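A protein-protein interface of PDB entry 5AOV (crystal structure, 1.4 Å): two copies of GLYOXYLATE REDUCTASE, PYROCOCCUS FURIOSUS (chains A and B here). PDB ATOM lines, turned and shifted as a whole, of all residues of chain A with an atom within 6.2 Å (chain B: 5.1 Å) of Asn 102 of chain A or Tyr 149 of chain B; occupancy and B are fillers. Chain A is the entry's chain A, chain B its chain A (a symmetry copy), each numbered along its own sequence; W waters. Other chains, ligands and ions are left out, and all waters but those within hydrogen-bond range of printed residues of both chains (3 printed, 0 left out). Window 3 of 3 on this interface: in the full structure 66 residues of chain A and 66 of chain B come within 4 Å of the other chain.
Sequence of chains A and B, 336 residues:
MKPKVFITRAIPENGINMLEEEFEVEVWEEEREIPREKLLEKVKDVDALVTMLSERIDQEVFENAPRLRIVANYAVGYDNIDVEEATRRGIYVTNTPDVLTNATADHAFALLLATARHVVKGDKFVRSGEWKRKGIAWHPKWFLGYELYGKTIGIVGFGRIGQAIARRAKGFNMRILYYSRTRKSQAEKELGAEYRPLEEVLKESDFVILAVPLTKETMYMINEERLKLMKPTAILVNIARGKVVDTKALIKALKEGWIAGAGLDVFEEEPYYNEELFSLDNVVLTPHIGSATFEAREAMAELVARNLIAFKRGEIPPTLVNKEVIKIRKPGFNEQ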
ATOM      1  N   ASP A  98      17.854  23.718  -0.631  1.00  0.00           N
ATOM      2  CA  ASP A  98      17.239  22.493  -0.092  1.00  0.00           C
ATOM      3  C   ASP A  98      17.263  22.372   1.453  1.00  0.00           C
ATOM      4  O   ASP A  98      16.282  22.097   2.078  1.00  0.00           O
ATOM      5  CB  ASP A  98      17.788  21.226  -0.746  1.00  0.00           C
ATOM      6  CG  ASP A  98      17.650  21.246  -2.275  1.00  0.00           C
ATOM      7  OD1 ASP A  98      16.507  21.352  -2.712  1.00  0.00           O
ATOM      8  OD2 ASP A  98      18.644  21.060  -2.961  1.00  0.00           O
ATOM      9  N   VAL A  99      18.474  22.572   2.004  1.00  0.00           N
ATOM     10  CA  VAL A  99      18.671  22.421   3.423  1.00  0.00           C
ATOM     11  C   VAL A  99      17.978  23.467   4.267  1.00  0.00           C
ATOM     12  O   VAL A  99      17.757  23.196   5.461  1.00  0.00           O
ATOM     13  CB  VAL A  99      20.174  22.425   3.744  1.00  0.00           C
ATOM     14  CG1 VAL A  99      20.917  21.272   3.094  1.00  0.00           C
ATOM     15  CG2 VAL A  99      20.865  23.727   3.312  1.00  0.00           C
ATOM     16  N   LEU A 100      17.522  24.565   3.660  1.00  0.00           N
ATOM     17  CA  LEU A 100      16.769  25.581   4.341  1.00  0.00           C
ATOM     18  C   LEU A 100      15.341  25.735   3.802  1.00  0.00           C
ATOM     19  O   LEU A 100      14.624  26.670   4.177  1.00  0.00           O
ATOM     20  CB  LEU A 100      17.500  26.942   4.293  1.00  0.00           C
ATOM     21  CG  LEU A 100      18.121  27.357   2.951  1.00  0.00           C
ATOM     22  CD1 LEU A 100      17.117  27.389   1.833  1.00  0.00           C
ATOM     23  CD2 LEU A 100      18.806  28.695   3.107  1.00  0.00           C
ATOM     24  N   THR A 101      14.911  24.829   2.923  1.00  0.00           N
ATOM     25  CA  THR A 101      13.562  24.948   2.306  1.00  0.00           C
ATOM     26  C   THR A 101      12.471  24.881   3.349  1.00  0.00           C
ATOM     27  O   THR A 101      11.553  25.707   3.314  1.00  0.00           O
ATOM     28  CB  THR A 101      13.382  23.850   1.308  1.00  0.00           C
ATOM     29  OG1 THR A 101      14.270  24.023   0.191  1.00  0.00           O
ATOM     30  CG2 THR A 101      11.951  23.779   0.764  1.00  0.00           C
ATOM     31  N   ASN A 102      12.550  23.909   4.223  1.00  0.00           N
ATOM     32  CA  ASN A 102      11.469  23.727   5.170  1.00  0.00           C
ATOM     33  C   ASN A 102      11.418  24.831   6.213  1.00  0.00           C
ATOM     34  O   ASN A 102      10.291  25.276   6.548  1.00  0.00           O
ATOM     35  CB  ASN A 102      11.516  22.329   5.737  1.00  0.00           C
ATOM     36  CG  ASN A 102      11.096  21.298   4.745  1.00  0.00           C
ATOM     37  OD1 ASN A 102      10.000  21.378   4.213  1.00  0.00           O
ATOM     38  ND2 ASN A 102      11.939  20.303   4.547  1.00  0.00           N
ATOM     39  N   ALA A 103      12.589  25.328   6.621  1.00  0.00           N
ATOM     40  CA  ALA A 103      12.600  26.441   7.590  1.00  0.00           C
ATOM     41  C   ALA A 103      11.910  27.643   6.999  1.00  0.00           C
ATOM     42  O   ALA A 103      11.089  28.322   7.643  1.00  0.00           O
ATOM     43  CB  ALA A 103      14.043  26.763   7.957  1.00  0.00           C
ATOM     44  N   THR A 104      12.222  27.966   5.750  1.00  0.00           N
ATOM     45  CA  THR A 104      11.752  29.192   5.176  1.00  0.00           C
ATOM     46  C   THR A 104      10.269  29.092   4.847  1.00  0.00           C
ATOM     47  O   THR A 104       9.506  30.068   4.996  1.00  0.00           O
ATOM     48  CB  THR A 104      12.583  29.592   3.944  1.00  0.00           C
ATOM     49  OG1 THR A 104      13.968  29.573   4.276  1.00  0.00           O
ATOM     50  CG2 THR A 104      12.242  30.990   3.528  1.00  0.00           C
ATOM     51  N   ALA A 105       9.828  27.941   4.351  1.00  0.00           N
ATOM     52  CA  ALA A 105       8.422  27.702   4.091  1.00  0.00           C
ATOM     53  C   ALA A 105       7.617  27.749   5.394  1.00  0.00           C
ATOM     54  O   ALA A 105       6.517  28.332   5.408  1.00  0.00           O
ATOM     55  CB  ALA A 105       8.209  26.402   3.353  1.00  0.00           C
ATOM     56  N   ASP A 106       8.165  27.216   6.482  1.00  0.00           N
ATOM     57  CA  ASP A 106       7.502  27.360   7.785  1.00  0.00           C
ATOM     58  C   ASP A 106       7.400  28.804   8.184  1.00  0.00           C
ATOM     59  O   ASP A 106       6.359  29.252   8.690  1.00  0.00           O
ATOM     60  CB  ASP A 106       8.253  26.624   8.895  1.00  0.00           C
ATOM     61  CG  ASP A 106       8.235  25.123   8.810  1.00  0.00           C
ATOM     62  OD1 ASP A 106       7.502  24.523   7.972  1.00  0.00           O
ATOM     63  OD2 ASP A 106       8.945  24.493   9.616  1.00  0.00           O
ATOM     64  N   HIS A 107       8.457  29.586   7.979  1.00  0.00           N
ATOM     65  CA  HIS A 107       8.432  30.990   8.385  1.00  0.00           C
ATOM     66  C   HIS A 107       7.481  31.771   7.531  1.00  0.00           C
ATOM     67  O   HIS A 107       6.801  32.711   8.031  1.00  0.00           O
ATOM     68  CB  HIS A 107       9.826  31.595   8.282  1.00  0.00           C
ATOM     69  CG  HIS A 107       9.918  32.843   9.123  1.00  0.00           C
ATOM     70  ND1 HIS A 107       9.779  32.800  10.498  1.00  0.00           N
ATOM     71  CD2 HIS A 107      10.085  34.145   8.775  1.00  0.00           C
ATOM     72  CE1 HIS A 107       9.890  34.056  10.957  1.00  0.00           C
ATOM     73  NE2 HIS A 107      10.030  34.873   9.919  1.00  0.00           N
ATOM     74  N   ILE A 161      11.162  26.687  -2.319  1.00  0.00           N
ATOM     75  CA  ILE A 161      10.406  27.219  -1.223  1.00  0.00           C
ATOM     76  C   ILE A 161       8.961  27.475  -1.620  1.00  0.00           C
ATOM     77  O   ILE A 161       8.064  27.120  -0.846  1.00  0.00           O
ATOM     78  CB  ILE A 161      11.136  28.480  -0.661  1.00  0.00           C
ATOM     79  CG1 ILE A 161      12.415  28.024   0.033  1.00  0.00           C
ATOM     80  CG2 ILE A 161      10.219  29.181   0.329  1.00  0.00           C
ATOM     81  CD1 ILE A 161      13.399  29.131   0.307  1.00  0.00           C
ATOM     82  N   ALA A 164       7.206  24.193  -1.452  1.00  0.00           N
ATOM     83  CA  ALA A 164       7.026  23.779  -0.073  1.00  0.00           C
ATOM     84  C   ALA A 164       5.933  24.585   0.658  1.00  0.00           C
ATOM     85  O   ALA A 164       5.177  24.017   1.483  1.00  0.00           O
ATOM     86  CB  ALA A 164       8.372  23.913   0.674  1.00  0.00           C
ATOM     87  N   ARG A 167       2.771  22.954  -0.462  1.00  0.00           N
ATOM     88  CA  ARG A 167       2.532  21.726   0.227  1.00  0.00           C
ATOM     89  C   ARG A 167       1.836  21.985   1.565  1.00  0.00           C
ATOM     90  O   ARG A 167       0.912  21.272   1.985  1.00  0.00           O
ATOM     91  CB  ARG A 167       3.843  20.953   0.456  1.00  0.00           C
ATOM     92  CG  ARG A 167       3.765  19.596   0.869  1.00  0.00           C
ATOM     93  CD  ARG A 167       5.216  18.920   0.556  1.00  0.00           C
ATOM     94  NE  ARG A 167       5.654  19.012  -0.857  1.00  0.00           N
ATOM     95  CZ  ARG A 167       6.696  19.701  -1.367  1.00  0.00           C
ATOM     96  NH1 ARG A 167       7.564  20.419  -0.663  1.00  0.00           N
ATOM     97  NH2 ARG A 167       6.903  19.661  -2.658  1.00  0.00           N
ATOM     98  N   ARG A 168       2.302  23.005   2.290  1.00  0.00           N
ATOM     99  CA  ARG A 168       1.704  23.364   3.555  1.00  0.00           C
ATOM    100  C   ARG A 168       0.289  23.884   3.306  1.00  0.00           C
ATOM    101  O   ARG A 168      -0.618  23.490   4.112  1.00  0.00           O
ATOM    102  CB  ARG A 168       2.567  24.403   4.289  1.00  0.00           C
ATOM    103  CG  ARG A 168       3.832  23.777   4.824  1.00  0.00           C
ATOM    104  CD  ARG A 168       4.960  24.851   4.916  1.00  0.00           C
ATOM    105  NE  ARG A 168       6.161  24.303   5.510  1.00  0.00           N
ATOM    106  CZ  ARG A 168       6.938  23.350   5.003  1.00  0.00           C
ATOM    107  NH1 ARG A 168       6.721  22.955   3.725  1.00  0.00           N
ATOM    108  NH2 ARG A 168       7.918  22.817   5.682  1.00  0.00           N
ATOM    109  N   GLY A 290      14.052  33.875   8.076  1.00  0.00           N
ATOM    110  CA  GLY A 290      13.367  32.740   7.430  1.00  0.00           C
ATOM    111  C   GLY A 290      14.081  31.427   7.566  1.00  0.00           C
ATOM    112  O   GLY A 290      13.438  30.419   7.775  1.00  0.00           O
ATOM    113  N   GLU B 147      12.345  23.361  13.565  1.00  0.00           N
ATOM    114  CA  GLU B 147      11.673  22.797  12.374  1.00  0.00           C
ATOM    115  C   GLU B 147      10.413  22.069  12.781  1.00  0.00           C
ATOM    116  O   GLU B 147      10.275  21.571  13.902  1.00  0.00           O
ATOM    117  CB  GLU B 147      12.596  21.783  11.733  1.00  0.00           C
ATOM    118  CG  GLU B 147      13.957  22.277  11.235  1.00  0.00           C
ATOM    119  CD  GLU B 147      13.928  22.731   9.805  1.00  0.00           C
ATOM    120  OE1 GLU B 147      13.202  22.072   9.016  1.00  0.00           O
ATOM    121  OE2 GLU B 147      14.793  23.458   9.334  1.00  0.00           O
ATOM    122  N   LEU B 148       9.506  22.010  11.818  1.00  0.00           N
ATOM    123  CA  LEU B 148       8.323  21.128  11.883  1.00  0.00           C
ATOM    124  C   LEU B 148       8.427  19.898  11.022  1.00  0.00           C
ATOM    125  O   LEU B 148       7.863  18.847  11.358  1.00  0.00           O
ATOM    126  CB  LEU B 148       7.038  21.878  11.498  1.00  0.00           C
ATOM    127  CG  LEU B 148       6.424  22.774  12.566  1.00  0.00           C
ATOM    128  CD1 LEU B 148       7.291  23.980  12.946  1.00  0.00           C
ATOM    129  CD2 LEU B 148       5.069  23.264  12.043  1.00  0.00           C
ATOM    130  N   TYR B 149       9.115  19.990   9.901  1.00  0.00           N
ATOM    131  CA  TYR B 149       9.115  18.920   8.926  1.00  0.00           C
ATOM    132  C   TYR B 149       9.696  17.671   9.491  1.00  0.00           C
ATOM    133  O   TYR B 149      10.843  17.627   9.990  1.00  0.00           O
ATOM    134  CB  TYR B 149       9.885  19.371   7.634  1.00  0.00           C
ATOM    135  CG  TYR B 149       9.932  18.386   6.499  1.00  0.00           C
ATOM    136  CD1 TYR B 149      10.915  17.449   6.428  1.00  0.00           C
ATOM    137  CD2 TYR B 149       8.990  18.429   5.477  1.00  0.00           C
ATOM    138  CE1 TYR B 149      10.946  16.540   5.326  1.00  0.00           C
ATOM    139  CE2 TYR B 149       9.042  17.579   4.416  1.00  0.00           C
ATOM    140  CZ  TYR B 149      10.004  16.657   4.374  1.00  0.00           C
ATOM    141  OH  TYR B 149      10.064  15.766   3.278  1.00  0.00           O
ATOM    142  N   GLY B 150       8.947  16.566   9.413  1.00  0.00           N
ATOM    143  CA  GLY B 150       9.440  15.301   9.936  1.00  0.00           C
ATOM    144  C   GLY B 150       9.323  15.157  11.472  1.00  0.00           C
ATOM    145  O   GLY B 150       9.789  14.127  12.003  1.00  0.00           O
ATOM    146  N   LYS B 151       8.886  16.202  12.157  1.00  0.00           N
ATOM    147  CA  LYS B 151       8.842  16.238  13.601  1.00  0.00           C
ATOM    148  C   LYS B 151       7.491  15.671  14.086  1.00  0.00           C
ATOM    149  O   LYS B 151       6.590  15.426  13.265  1.00  0.00           O
ATOM    150  CB  LYS B 151       9.071  17.644  14.146  1.00  0.00           C
ATOM    151  CG  LYS B 151      10.392  18.254  13.673  1.00  0.00           C
ATOM    152  CD  LYS B 151      11.582  17.546  14.299  1.00  0.00           C
ATOM    153  CE  LYS B 151      12.850  18.255  13.847  1.00  0.00           C
ATOM    154  NZ  LYS B 151      14.056  17.554  14.378  1.00  0.00           N
ATOM    155  N   PHE B 172       2.931  19.757   6.654  1.00  0.00           N
ATOM    156  CA  PHE B 172       4.292  19.919   7.153  1.00  0.00           C
ATOM    157  C   PHE B 172       5.001  18.568   7.291  1.00  0.00           C
ATOM    158  O   PHE B 172       6.084  18.553   7.860  1.00  0.00           O
ATOM    159  CB  PHE B 172       4.259  20.659   8.476  1.00  0.00           C
ATOM    160  CG  PHE B 172       3.765  22.107   8.402  1.00  0.00           C
ATOM    161  CD1 PHE B 172       2.401  22.375   8.352  1.00  0.00           C
ATOM    162  CD2 PHE B 172       4.653  23.189   8.425  1.00  0.00           C
ATOM    163  CE1 PHE B 172       1.911  23.656   8.307  1.00  0.00           C
ATOM    164  CE2 PHE B 172       4.176  24.490   8.365  1.00  0.00           C
ATOM    165  CZ  PHE B 172       2.851  24.751   8.303  1.00  0.00           C
ATOM    166  N   ASN B 173       4.402  17.517   6.816  1.00  0.00           N
ATOM    167  CA  ASN B 173       5.027  16.193   6.901  1.00  0.00           C
ATOM    168  C   ASN B 173       5.361  15.828   8.329  1.00  0.00           C
ATOM    169  O   ASN B 173       6.488  15.327   8.615  1.00  0.00           O
ATOM    170  CB  ASN B 173       6.315  16.113   6.075  1.00  0.00           C
ATOM    171  CG  ASN B 173       6.880  14.677   6.000  1.00  0.00           C
ATOM    172  OD1 ASN B 173       6.159  13.711   5.917  1.00  0.00           O
ATOM    173  ND2 ASN B 173       8.193  14.587   6.084  1.00  0.00           N
HETATM  174  O   HOH W   1      14.295  20.396   6.881  1.00  0.00           O
HETATM  175  O   HOH W   2      10.334  22.374   8.870  1.00  0.00           O
HETATM  176  O   HOH W   3      15.018  23.743   6.629  1.00  0.00           O
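Water W2 lies within hydrogen-bond range of OD2 of Asp 106 of chain A, N of Tyr 149 of chain B, OE1 of Glu 147 of chain B and N of Leu 148 of chain B.
Water W3 lies within hydrogen-bond range of the side-chain carboxylate of Glu 147 of chain B (2.7 Å), the backbone NH of Ala 103 of chain A (2.9 Å), the backbone carbonyl oxygen of Val 99 of chain A (3.0 Å) and the backbone NH of Asn 102 of chain A (3.5 Å).
Water W1 bridges the side-chain carboxylate of Glu 147 of chain B (2.9 Å) and the side-chain amide nitrogen of Asn 102 of chain A (3.3 Å).
Asn 102 of chain A touches Glu 147 of chain B.
OD1 of Asn 102 of chain A touches CD2 of Tyr 149 of chain B, at 3.4 Å.
Ala 103 of chain A touches Glu 147 of chain B (CB to OE2, 3.7 Å).
Asp 106 of chain A touches Phe 172 of chain B.
NE of Arg 168 of chain A touches CD2 of Phe 172 of chain B, at 3.5 Å.
The side-chain carboxylate (OD2) of Asp 106 of chain A is in hydrogen-bond range of the backbone NH (N) of Leu 148 of chain B (3.4 Å).
Hydrophobic or aromatic side chains of chain A within 4 Å of the printed part of chain B: Ala 103.
Printed residues of chain B that touch a printed residue of chain A: Glu 147, Leu 148, Tyr 149 and Phe 172.
Hydrophobic or aromatic side chains of chain B within 4 Å of the printed part of chain A: Leu 148, Tyr 149 and Phe 172.
Among the printed residues, 6 pairs touch across the chains.
Of chain B, only Glu 147 and Tyr 149 come within 4 Å of Asn 102 of chain A.
Of the printed residues of chain B, Ala 103 of chain A touches Glu 147 (3.7 Å).
Of the printed residues of chain B, Asp 106 of chain A touches Leu 148 (3.4 Å) and Phe 172 (3.2 Å).
Tyr 149 of chain B touches one residue of chain A.
Lys 151 of chain B touches none of the printed residues of chain A.
The nearest printed residue of chain B that does not touch Asn 102 of chain A is Phe 172 of chain B (6.1 Å).
No position is printed for both chains.
Of the 6 pairs that touch across the chains among the printed residues, none has its exchanged pair printed and touching as well.
NH1 of Arg 168 of chain A sits at hydrogen-bond distance from O of Ala 164 of chain A (2.9 Å).
OD1 of Asp 106 of chain A lies within salt-bridge range of NE of Arg 168 of chain A (2.8 Å).
The side-chain amide oxygen (OD1) of Asn 102 of chain A lies within hydrogen-bond range of the guanidinium group (NH2) of Arg 168 of chain A (2.9 Å).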
